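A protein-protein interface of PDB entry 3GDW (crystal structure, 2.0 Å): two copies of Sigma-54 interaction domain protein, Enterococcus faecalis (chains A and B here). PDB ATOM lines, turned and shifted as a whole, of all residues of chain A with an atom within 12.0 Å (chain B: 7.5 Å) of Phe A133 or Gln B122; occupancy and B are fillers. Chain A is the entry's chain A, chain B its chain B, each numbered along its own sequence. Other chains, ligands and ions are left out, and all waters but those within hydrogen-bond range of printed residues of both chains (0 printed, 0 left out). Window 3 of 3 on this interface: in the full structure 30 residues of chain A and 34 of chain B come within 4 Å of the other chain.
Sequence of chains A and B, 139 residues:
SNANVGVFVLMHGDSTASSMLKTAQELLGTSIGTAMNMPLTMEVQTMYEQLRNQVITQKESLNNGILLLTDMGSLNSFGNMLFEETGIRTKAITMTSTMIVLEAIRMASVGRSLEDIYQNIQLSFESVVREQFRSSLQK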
ATOM      1  N   MET A  95      25.406 -25.597  -3.271  1.00  0.00           N
ATOM      2  CA  MET A  95      24.924 -24.883  -4.450  1.00  0.00           C
ATOM      3  C   MET A  95      23.582 -25.453  -4.917  1.00  0.00           C
ATOM      4  O   MET A  95      23.356 -25.691  -6.081  1.00  0.00           O
ATOM      5  CB  MET A  95      25.988 -24.821  -5.566  1.00  0.00           C
ATOM      6  CG  MET A  95      26.017 -23.427  -6.241  1.00  0.00           C
ATOM      7  SD  MET A  95      27.298 -23.432  -7.641  1.00  0.00           S
ATOM      8  CE  MET A  95      28.712 -22.507  -6.637  1.00  0.00           C
ATOM      9  N   SER A  97      19.912 -25.833  -6.080  1.00  0.00           N
ATOM     10  CA  SER A  97      18.911 -25.087  -6.860  1.00  0.00           C
ATOM     11  C   SER A  97      17.654 -25.921  -6.976  1.00  0.00           C
ATOM     12  O   SER A  97      17.634 -27.067  -6.546  1.00  0.00           O
ATOM     13  CB  SER A  97      19.449 -24.776  -8.262  1.00  0.00           C
ATOM     14  OG  SER A  97      19.847 -25.971  -8.919  1.00  0.00           O
ATOM     15  N   SER A 124      24.039 -35.678 -12.385  1.00  0.00           N
ATOM     16  CA  SER A 124      23.144 -34.740 -13.092  1.00  0.00           C
ATOM     17  C   SER A 124      23.689 -33.325 -13.039  1.00  0.00           C
ATOM     18  O   SER A 124      23.672 -32.594 -14.034  1.00  0.00           O
ATOM     19  CB  SER A 124      21.746 -34.696 -12.461  1.00  0.00           C
ATOM     20  OG  SER A 124      21.084 -35.949 -12.577  1.00  0.00           O
ATOM     21  N   PHE A 125      24.137 -32.932 -11.857  1.00  0.00           N
ATOM     22  CA  PHE A 125      24.668 -31.597 -11.677  1.00  0.00           C
ATOM     23  C   PHE A 125      25.873 -31.406 -12.611  1.00  0.00           C
ATOM     24  O   PHE A 125      25.976 -30.404 -13.313  1.00  0.00           O
ATOM     25  CB  PHE A 125      25.046 -31.364 -10.227  1.00  0.00           C
ATOM     26  CG  PHE A 125      25.613 -30.009  -9.957  1.00  0.00           C
ATOM     27  CD1 PHE A 125      24.783 -28.893  -9.829  1.00  0.00           C
ATOM     28  CD2 PHE A 125      26.987 -29.841  -9.825  1.00  0.00           C
ATOM     29  CE1 PHE A 125      25.335 -27.624  -9.568  1.00  0.00           C
ATOM     30  CE2 PHE A 125      27.556 -28.596  -9.588  1.00  0.00           C
ATOM     31  CZ  PHE A 125      26.736 -27.483  -9.440  1.00  0.00           C
ATOM     32  N   GLU A 126      26.765 -32.383 -12.645  1.00  0.00           N
ATOM     33  CA  GLU A 126      27.954 -32.264 -13.480  1.00  0.00           C
ATOM     34  C   GLU A 126      27.580 -32.251 -14.965  1.00  0.00           C
ATOM     35  O   GLU A 126      28.162 -31.516 -15.753  1.00  0.00           O
ATOM     36  CB  GLU A 126      28.932 -33.388 -13.161  1.00  0.00           C
ATOM     37  CG  GLU A 126      30.327 -33.177 -13.725  1.00  0.00           C
ATOM     38  CD  GLU A 126      30.425 -33.511 -15.199  1.00  0.00           C
ATOM     39  OE1 GLU A 126      29.595 -34.320 -15.673  1.00  0.00           O
ATOM     40  OE2 GLU A 126      31.326 -32.972 -15.885  1.00  0.00           O
ATOM     41  N   SER A 127      26.608 -33.065 -15.356  1.00  0.00           N
ATOM     42  CA  SER A 127      26.195 -33.084 -16.743  1.00  0.00           C
ATOM     43  C   SER A 127      25.687 -31.725 -17.230  1.00  0.00           C
ATOM     44  O   SER A 127      26.048 -31.270 -18.329  1.00  0.00           O
ATOM     45  CB  SER A 127      25.122 -34.140 -16.980  1.00  0.00           C
ATOM     46  OG  SER A 127      25.065 -34.402 -18.371  1.00  0.00           O
ATOM     47  N   VAL A 128      24.849 -31.094 -16.408  1.00  0.00           N
ATOM     48  CA  VAL A 128      24.183 -29.857 -16.783  1.00  0.00           C
ATOM     49  C   VAL A 128      25.188 -28.717 -16.840  1.00  0.00           C
ATOM     50  O   VAL A 128      25.132 -27.900 -17.757  1.00  0.00           O
ATOM     51  CB  VAL A 128      23.015 -29.519 -15.827  1.00  0.00           C
ATOM     52  CG1 VAL A 128      22.440 -28.161 -16.153  1.00  0.00           C
ATOM     53  CG2 VAL A 128      21.919 -30.597 -15.955  1.00  0.00           C
ATOM     54  N   VAL A 129      26.088 -28.673 -15.851  1.00  0.00           N
ATOM     55  CA  VAL A 129      27.210 -27.724 -15.854  1.00  0.00           C
ATOM     56  C   VAL A 129      28.015 -27.824 -17.154  1.00  0.00           C
ATOM     57  O   VAL A 129      28.237 -26.814 -17.830  1.00  0.00           O
ATOM     58  CB  VAL A 129      28.150 -27.893 -14.645  1.00  0.00           C
ATOM     59  CG1 VAL A 129      29.459 -27.112 -14.878  1.00  0.00           C
ATOM     60  CG2 VAL A 129      27.481 -27.387 -13.407  1.00  0.00           C
ATOM     61  N   ARG A 130      28.420 -29.045 -17.506  1.00  0.00           N
ATOM     62  CA  ARG A 130      29.232 -29.268 -18.688  1.00  0.00           C
ATOM     63  C   ARG A 130      28.496 -28.877 -19.976  1.00  0.00           C
ATOM     64  O   ARG A 130      29.103 -28.314 -20.893  1.00  0.00           O
ATOM     65  CB  ARG A 130      29.695 -30.717 -18.749  1.00  0.00           C
ATOM     66  CG  ARG A 130      30.713 -30.995 -19.840  1.00  0.00           C
ATOM     67  CD  ARG A 130      30.976 -32.495 -20.016  1.00  0.00           C
ATOM     68  NE  ARG A 130      29.736 -33.244 -20.254  1.00  0.00           N
ATOM     69  CZ  ARG A 130      29.228 -34.158 -19.428  1.00  0.00           C
ATOM     70  NH1 ARG A 130      29.862 -34.472 -18.307  1.00  0.00           N
ATOM     71  NH2 ARG A 130      28.086 -34.771 -19.731  1.00  0.00           N
ATOM     72  N   GLU A 131      27.200 -29.168 -20.053  1.00  0.00           N
ATOM     73  CA  GLU A 131      26.425 -28.735 -21.222  1.00  0.00           C
ATOM     74  C   GLU A 131      26.242 -27.212 -21.273  1.00  0.00           C
ATOM     75  O   GLU A 131      26.301 -26.620 -22.358  1.00  0.00           O
ATOM     76  CB  GLU A 131      25.080 -29.451 -21.310  1.00  0.00           C
ATOM     77  CG  GLU A 131      25.192 -30.895 -21.775  1.00  0.00           C
ATOM     78  CD  GLU A 131      26.162 -31.055 -22.933  1.00  0.00           C
ATOM     79  OE1 GLU A 131      25.983 -30.373 -23.972  1.00  0.00           O
ATOM     80  OE2 GLU A 131      27.109 -31.862 -22.808  1.00  0.00           O
ATOM     81  N   GLN A 132      26.014 -26.597 -20.109  1.00  0.00           N
ATOM     82  CA  GLN A 132      25.859 -25.141 -19.992  1.00  0.00           C
ATOM     83  C   GLN A 132      27.087 -24.388 -20.507  1.00  0.00           C
ATOM     84  O   GLN A 132      26.965 -23.406 -21.242  1.00  0.00           O
ATOM     85  CB  GLN A 132      25.580 -24.739 -18.539  1.00  0.00           C
ATOM     86  CG  GLN A 132      26.000 -23.310 -18.182  1.00  0.00           C
ATOM     87  CD  GLN A 132      24.979 -22.254 -18.590  1.00  0.00           C
ATOM     88  OE1 GLN A 132      25.308 -21.261 -19.260  1.00  0.00           O
ATOM     89  NE2 GLN A 132      23.736 -22.462 -18.183  1.00  0.00           N
ATOM     90  N   PHE A 133      28.268 -24.854 -20.118  1.00  0.00           N
ATOM     91  CA  PHE A 133      29.493 -24.145 -20.458  1.00  0.00           C
ATOM     92  C   PHE A 133      30.236 -24.725 -21.661  1.00  0.00           C
ATOM     93  O   PHE A 133      31.359 -24.320 -21.949  1.00  0.00           O
ATOM     94  CB  PHE A 133      30.379 -24.025 -19.219  1.00  0.00           C
ATOM     95  CG  PHE A 133      29.755 -23.212 -18.130  1.00  0.00           C
ATOM     96  CD1 PHE A 133      29.576 -21.852 -18.293  1.00  0.00           C
ATOM     97  CD2 PHE A 133      29.333 -23.814 -16.943  1.00  0.00           C
ATOM     98  CE1 PHE A 133      28.990 -21.092 -17.311  1.00  0.00           C
ATOM     99  CE2 PHE A 133      28.760 -23.063 -15.948  1.00  0.00           C
ATOM    100  CZ  PHE A 133      28.573 -21.695 -16.131  1.00  0.00           C
ATOM    101  N   ARG A 134      29.585 -25.644 -22.376  1.00  0.00           N
ATOM    102  CA  ARG A 134      30.182 -26.320 -23.541  1.00  0.00           C
ATOM    103  C   ARG A 134      30.648 -25.377 -24.665  1.00  0.00           C
ATOM    104  O   ARG A 134      31.830 -25.408 -25.069  1.00  0.00           O
ATOM    105  CB  ARG A 134      29.226 -27.387 -24.102  1.00  0.00           C
ATOM    106  CG  ARG A 134      29.719 -28.067 -25.379  1.00  0.00           C
ATOM    107  CD  ARG A 134      28.821 -29.220 -25.824  1.00  0.00           C
ATOM    108  NE  ARG A 134      28.795 -30.275 -24.816  1.00  0.00           N
ATOM    109  CZ  ARG A 134      29.770 -31.162 -24.636  1.00  0.00           C
ATOM    110  NH1 ARG A 134      30.855 -31.132 -25.404  1.00  0.00           N
ATOM    111  NH2 ARG A 134      29.664 -32.078 -23.682  1.00  0.00           N
ATOM    112  N   SER A 135      29.734 -24.559 -25.182  1.00  0.00           N
ATOM    113  CA  SER A 135      29.978 -23.849 -26.451  1.00  0.00           C
ATOM    114  C   SER A 135      29.785 -22.340 -26.346  1.00  0.00           C
ATOM    115  O   SER A 135      30.156 -21.595 -27.264  1.00  0.00           O
ATOM    116  CB  SER A 135      29.106 -24.429 -27.575  1.00  0.00           C
ATOM    117  N   ALA B  92      22.911 -16.610 -20.526  1.00  0.00           N
ATOM    118  CA  ALA B  92      21.987 -17.273 -19.605  1.00  0.00           C
ATOM    119  C   ALA B  92      22.689 -18.424 -18.861  1.00  0.00           C
ATOM    120  O   ALA B  92      23.438 -19.195 -19.454  1.00  0.00           O
ATOM    121  CB  ALA B  92      20.770 -17.791 -20.358  1.00  0.00           C
ATOM    122  N   ILE B  93      22.467 -18.508 -17.557  1.00  0.00           N
ATOM    123  CA  ILE B  93      23.102 -19.539 -16.744  1.00  0.00           C
ATOM    124  C   ILE B  93      22.027 -20.269 -15.944  1.00  0.00           C
ATOM    125  O   ILE B  93      21.275 -19.629 -15.204  1.00  0.00           O
ATOM    126  CB  ILE B  93      24.160 -18.896 -15.796  1.00  0.00           C
ATOM    127  CG1 ILE B  93      25.349 -18.399 -16.632  1.00  0.00           C
ATOM    128  CG2 ILE B  93      24.609 -19.877 -14.695  1.00  0.00           C
ATOM    129  CD1 ILE B  93      26.354 -17.558 -15.875  1.00  0.00           C
ATOM    130  N   THR B  94      21.969 -21.597 -16.109  1.00  0.00           N
ATOM    131  CA  THR B  94      21.061 -22.479 -15.361  1.00  0.00           C
ATOM    132  C   THR B  94      21.648 -22.919 -14.015  1.00  0.00           C
ATOM    133  O   THR B  94      22.817 -22.660 -13.728  1.00  0.00           O
ATOM    134  CB  THR B  94      20.728 -23.785 -16.149  1.00  0.00           C
ATOM    135  OG1 THR B  94      21.922 -24.543 -16.374  1.00  0.00           O
ATOM    136  CG2 THR B  94      20.091 -23.483 -17.468  1.00  0.00           C
ATOM    137  N   ILE B 100      25.734 -17.829  -6.601  1.00  0.00           N
ATOM    138  CA  ILE B 100      25.823 -17.392  -7.990  1.00  0.00           C
ATOM    139  C   ILE B 100      25.106 -16.048  -8.153  1.00  0.00           C
ATOM    140  O   ILE B 100      25.662 -15.153  -8.780  1.00  0.00           O
ATOM    141  CB  ILE B 100      25.217 -18.432  -8.976  1.00  0.00           C
ATOM    142  CG1 ILE B 100      25.944 -19.777  -8.878  1.00  0.00           C
ATOM    143  CG2 ILE B 100      25.327 -17.928 -10.397  1.00  0.00           C
ATOM    144  CD1 ILE B 100      27.470 -19.633  -8.940  1.00  0.00           C
ATOM    145  N   MET B 107      29.682  -8.478  -8.878  1.00  0.00           N
ATOM    146  CA  MET B 107      30.510  -8.108 -10.019  1.00  0.00           C
ATOM    147  C   MET B 107      29.824  -7.096 -10.929  1.00  0.00           C
ATOM    148  O   MET B 107      30.463  -6.118 -11.356  1.00  0.00           O
ATOM    149  CB  MET B 107      30.936  -9.346 -10.800  1.00  0.00           C
ATOM    150  CG  MET B 107      31.814 -10.248  -9.987  1.00  0.00           C
ATOM    151  SD  MET B 107      32.468 -11.775 -10.990  1.00  0.00           S
ATOM    152  CE  MET B 107      30.879 -12.821 -11.225  1.00  0.00           C
ATOM    153  N   ASP B 116      33.377 -11.306 -18.206  1.00  0.00           N
ATOM    154  CA  ASP B 116      34.153 -11.477 -16.973  1.00  0.00           C
ATOM    155  C   ASP B 116      33.300 -12.131 -15.882  1.00  0.00           C
ATOM    156  O   ASP B 116      33.771 -13.011 -15.154  1.00  0.00           O
ATOM    157  CB  ASP B 116      34.699 -10.108 -16.527  1.00  0.00           C
ATOM    158  CG  ASP B 116      35.684 -10.200 -15.372  1.00  0.00           C
ATOM    159  OD1 ASP B 116      35.931 -11.309 -14.863  1.00  0.00           O
ATOM    160  OD2 ASP B 116      36.213  -9.145 -14.963  1.00  0.00           O
ATOM    161  N   ILE B 117      32.036 -11.714 -15.794  1.00  0.00           N
ATOM    162  CA  ILE B 117      31.084 -12.272 -14.862  1.00  0.00           C
ATOM    163  C   ILE B 117      30.782 -13.726 -15.215  1.00  0.00           C
ATOM    164  O   ILE B 117      30.791 -14.599 -14.343  1.00  0.00           O
ATOM    165  CB  ILE B 117      29.751 -11.466 -14.800  1.00  0.00           C
ATOM    166  CG1 ILE B 117      29.994 -10.041 -14.266  1.00  0.00           C
ATOM    167  CG2 ILE B 117      28.747 -12.232 -13.905  1.00  0.00           C
ATOM    168  CD1 ILE B 117      28.792  -9.056 -14.488  1.00  0.00           C
ATOM    169  N   TYR B 118      30.535 -13.977 -16.501  1.00  0.00           N
ATOM    170  CA  TYR B 118      30.215 -15.322 -16.990  1.00  0.00           C
ATOM    171  C   TYR B 118      31.358 -16.307 -16.707  1.00  0.00           C
ATOM    172  O   TYR B 118      31.110 -17.454 -16.308  1.00  0.00           O
ATOM    173  CB  TYR B 118      29.909 -15.276 -18.497  1.00  0.00           C
ATOM    174  CG  TYR B 118      29.351 -16.587 -19.069  1.00  0.00           C
ATOM    175  CD1 TYR B 118      27.993 -16.856 -19.020  1.00  0.00           C
ATOM    176  CD2 TYR B 118      30.188 -17.526 -19.691  1.00  0.00           C
ATOM    177  CE1 TYR B 118      27.461 -18.036 -19.539  1.00  0.00           C
ATOM    178  CE2 TYR B 118      29.667 -18.718 -20.214  1.00  0.00           C
ATOM    179  CZ  TYR B 118      28.307 -18.955 -20.144  1.00  0.00           C
ATOM    180  OH  TYR B 118      27.753 -20.100 -20.655  1.00  0.00           O
ATOM    181  N   GLN B 119      32.590 -15.854 -16.925  1.00  0.00           N
ATOM    182  CA  GLN B 119      33.783 -16.677 -16.673  1.00  0.00           C
ATOM    183  C   GLN B 119      33.926 -16.982 -15.205  1.00  0.00           C
ATOM    184  O   GLN B 119      34.161 -18.126 -14.852  1.00  0.00           O
ATOM    185  CB  GLN B 119      35.091 -16.023 -17.173  1.00  0.00           C
ATOM    186  CG  GLN B 119      36.347 -16.891 -16.806  1.00  0.00           C
ATOM    187  CD  GLN B 119      37.685 -16.200 -17.065  1.00  0.00           C
ATOM    188  OE1 GLN B 119      38.191 -16.215 -18.185  1.00  0.00           O
ATOM    189  NE2 GLN B 119      38.277 -15.623 -16.021  1.00  0.00           N
ATOM    190  N   ASN B 120      33.789 -15.971 -14.346  1.00  0.00           N
ATOM    191  CA  ASN B 120      33.905 -16.203 -12.891  1.00  0.00           C
ATOM    192  C   ASN B 120      32.817 -17.125 -12.337  1.00  0.00           C
ATOM    193  O   ASN B 120      33.056 -17.923 -11.415  1.00  0.00           O
ATOM    194  CB  ASN B 120      34.000 -14.890 -12.101  1.00  0.00           C
ATOM    195  CG  ASN B 120      35.402 -14.267 -12.165  1.00  0.00           C
ATOM    196  OD1 ASN B 120      36.235 -14.505 -11.290  1.00  0.00           O
ATOM    197  ND2 ASN B 120      35.672 -13.488 -13.210  1.00  0.00           N
ATOM    198  N   ILE B 121      31.623 -17.031 -12.912  1.00  0.00           N
ATOM    199  CA  ILE B 121      30.565 -17.921 -12.515  1.00  0.00           C
ATOM    200  C   ILE B 121      30.853 -19.352 -12.977  1.00  0.00           C
ATOM    201  O   ILE B 121      30.601 -20.314 -12.240  1.00  0.00           O
ATOM    202  CB  ILE B 121      29.180 -17.444 -13.004  1.00  0.00           C
ATOM    203  CG1 ILE B 121      28.713 -16.218 -12.185  1.00  0.00           C
ATOM    204  CG2 ILE B 121      28.168 -18.578 -12.845  1.00  0.00           C
ATOM    205  CD1 ILE B 121      27.418 -15.548 -12.702  1.00  0.00           C
ATOM    206  N   GLN B 122      31.362 -19.499 -14.199  1.00  0.00           N
ATOM    207  CA  GLN B 122      31.755 -20.818 -14.658  1.00  0.00           C
ATOM    208  C   GLN B 122      32.797 -21.423 -13.725  1.00  0.00           C
ATOM    209  O   GLN B 122      32.712 -22.580 -13.396  1.00  0.00           O
ATOM    210  CB  GLN B 122      32.269 -20.785 -16.097  1.00  0.00           C
ATOM    211  CG  GLN B 122      32.694 -22.162 -16.556  1.00  0.00           C
ATOM    212  CD  GLN B 122      33.189 -22.179 -18.001  1.00  0.00           C
ATOM    213  OE1 GLN B 122      33.118 -21.181 -18.710  1.00  0.00           O
ATOM    214  NE2 GLN B 122      33.649 -23.319 -18.438  1.00  0.00           N
ATOM    215  N   LEU B 123      33.778 -20.641 -13.283  1.00  0.00           N
ATOM    216  CA  LEU B 123      34.771 -21.155 -12.333  1.00  0.00           C
ATOM    217  C   LEU B 123      34.159 -21.594 -10.996  1.00  0.00           C
ATOM    218  O   LEU B 123      34.623 -22.575 -10.387  1.00  0.00           O
ATOM    219  CB  LEU B 123      35.885 -20.129 -12.107  1.00  0.00           C
ATOM    220  CG  LEU B 123      36.888 -19.969 -13.254  1.00  0.00           C
ATOM    221  CD1 LEU B 123      37.632 -18.625 -13.175  1.00  0.00           C
ATOM    222  CD2 LEU B 123      37.889 -21.158 -13.305  1.00  0.00           C
ATOM    223  N   SER B 124      33.126 -20.878 -10.533  1.00  0.00           N
ATOM    224  CA  SER B 124      32.436 -21.259  -9.324  1.00  0.00           C
ATOM    225  C   SER B 124      31.746 -22.599  -9.502  1.00  0.00           C
ATOM    226  O   SER B 124      31.840 -23.450  -8.641  1.00  0.00           O
ATOM    227  CB  SER B 124      31.408 -20.190  -8.911  1.00  0.00           C
ATOM    228  OG  SER B 124      32.059 -18.991  -8.496  1.00  0.00           O
ATOM    229  N   PHE B 125      31.045 -22.781 -10.618  1.00  0.00           N
ATOM    230  CA  PHE B 125      30.419 -24.057 -10.894  1.00  0.00           C
ATOM    231  C   PHE B 125      31.489 -25.156 -10.922  1.00  0.00           C
ATOM    232  O   PHE B 125      31.318 -26.184 -10.264  1.00  0.00           O
ATOM    233  CB  PHE B 125      29.601 -24.022 -12.188  1.00  0.00           C
ATOM    234  CG  PHE B 125      28.184 -23.521 -11.999  1.00  0.00           C
ATOM    235  CD1 PHE B 125      27.183 -24.362 -11.513  1.00  0.00           C
ATOM    236  CD2 PHE B 125      27.858 -22.221 -12.288  1.00  0.00           C
ATOM    237  CE1 PHE B 125      25.870 -23.900 -11.336  1.00  0.00           C
ATOM    238  CE2 PHE B 125      26.554 -21.753 -12.124  1.00  0.00           C
ATOM    239  CZ  PHE B 125      25.561 -22.597 -11.648  1.00  0.00           C
ATOM    240  N   GLU B 126      32.600 -24.914 -11.637  1.00  0.00           N
ATOM    241  CA  GLU B 126      33.682 -25.921 -11.741  1.00  0.00           C
ATOM    242  C   GLU B 126      34.258 -26.303 -10.396  1.00  0.00           C
ATOM    243  O   GLU B 126      34.504 -27.484 -10.168  1.00  0.00           O
ATOM    244  CB  GLU B 126      34.843 -25.483 -12.655  1.00  0.00           C
ATOM    245  CG  GLU B 126      34.414 -24.925 -13.978  1.00  0.00           C
ATOM    246  CD  GLU B 126      34.466 -25.931 -15.108  1.00  0.00           C
ATOM    247  OE1 GLU B 126      34.605 -27.153 -14.829  1.00  0.00           O
ATOM    248  OE2 GLU B 126      34.384 -25.474 -16.275  1.00  0.00           O
ATOM    249  N   SER B 127      34.465 -25.319  -9.512  1.00  0.00           N
ATOM    250  CA  SER B 127      34.935 -25.607  -8.156  1.00  0.00           C
ATOM    251  C   SER B 127      34.006 -26.577  -7.455  1.00  0.00           C
ATOM    252  O   SER B 127      34.469 -27.509  -6.808  1.00  0.00           O
ATOM    253  CB  SER B 127      35.041 -24.351  -7.307  1.00  0.00           C
ATOM    254  OG  SER B 127      35.909 -23.445  -7.913  1.00  0.00           O
ATOM    255  N   VAL B 128      32.694 -26.357  -7.582  1.00  0.00           N
ATOM    256  CA  VAL B 128      31.703 -27.218  -6.940  1.00  0.00           C
ATOM    257  C   VAL B 128      31.664 -28.633  -7.533  1.00  0.00           C
ATOM    258  O   VAL B 128      31.469 -29.605  -6.801  1.00  0.00           O
ATOM    259  CB  VAL B 128      30.278 -26.576  -6.972  1.00  0.00           C
ATOM    260  CG1 VAL B 128      29.182 -27.608  -6.557  1.00  0.00           C
ATOM    261  CG2 VAL B 128      30.250 -25.402  -6.039  1.00  0.00           C
ATOM    262  N   VAL B 129      31.804 -28.736  -8.851  1.00  0.00           N
ATOM    263  CA  VAL B 129      31.837 -30.029  -9.532  1.00  0.00           C
ATOM    264  C   VAL B 129      32.982 -30.861  -8.953  1.00  0.00           C
ATOM    265  O   VAL B 129      32.831 -32.058  -8.651  1.00  0.00           O
ATOM    266  CB  VAL B 129      31.980 -29.837 -11.059  1.00  0.00           C
ATOM    267  CG1 VAL B 129      32.318 -31.157 -11.789  1.00  0.00           C
ATOM    268  CG2 VAL B 129      30.704 -29.197 -11.612  1.00  0.00           C
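Of chain B, only Tyr B118 (3.5 Å), Gln B122 (3.4 Å) and Phe B125 (3.9 Å) come within 4 Å of Phe A133.
Of chain A, only Phe A133 (3.4 Å) comes within 4 Å of Gln B122.
No residue of chain A comes within 4 Å of Gln B119.
No residue of chain A comes within 4 Å of Asn B120.
Ile B121 touches none of the printed residues of chain A.
No residue of chain A comes within 4 Å of Glu B126.
Printed residues of chain A within 4 Å of Tyr B118: Gln A132 (3.0 Å) and Phe A133 (3.5 Å).
Of the printed residues of chain A, Ala B92 touches Gln A132 (2.8 Å).
The nearest residue of chain B that does not touch Phe A133 is Ile B121 (4.5 Å).
The nearest residue of chain A that does not touch Gln B122 is Val A129 (5.8 Å).
Phe A125 touches its own counterpart, Phe B125.
Phe A125 touches Val B128, but with the chains exchanged Val A128 does not touch Phe B125 (7.2 Å).
Phe A125 touches Val B129, and with the chains exchanged Val A129 touches Phe B125.
Glu A126 touches Val B129, but with the chains exchanged Val A129 does not touch Glu B126 (5.0 Å).
The backbone carbonyl oxygen (O) of Ala B92 lies close to the side-chain amide oxygen (OE1) of Gln A132.
NE2 of Gln A132 lies close to N of Thr B94.
The side-chain hydroxyl (OH) of Tyr B118 lies within hydrogen-bond range of the side-chain amide oxygen (OE1) of Gln A132, 3.0 Å away.
Hydrophobic or aromatic side chains of chain A within 4 Å of the printed part of chain B: Met A95, Phe A125, Val A128, Val A129 and Phe A133.
Among the printed residues, merely in contact across the chains: Met A95 with Ile B100, Met A95 with Ser B124, Met A95 with Phe B125, Met A95 with Val B128, Phe A125 with Phe B125, Phe A125 with Val B128, Phe A125 with Val B129, Glu A126 with Val B129, Val A128 with Thr B94, Val A129 with Phe B125, Gln A132 with Ile B93, Phe A133 with Tyr B118, Phe A133 with Gln B122 and Phe A133 with Phe B125.
The side-chain carboxylate (OE1) of Glu A126 lies within salt-bridge range of the guanidinium group (NH1) of Arg A130, 2.7 Å away.
OG of Ser B124 lies within hydrogen-bond range of O of Asn B120 (3.3 Å).
The side-chain carboxylate (OE2) of Glu B126 sits at hydrogen-bond distance from the side-chain amide nitrogen (NE2) of Gln B122 (3.1 Å).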
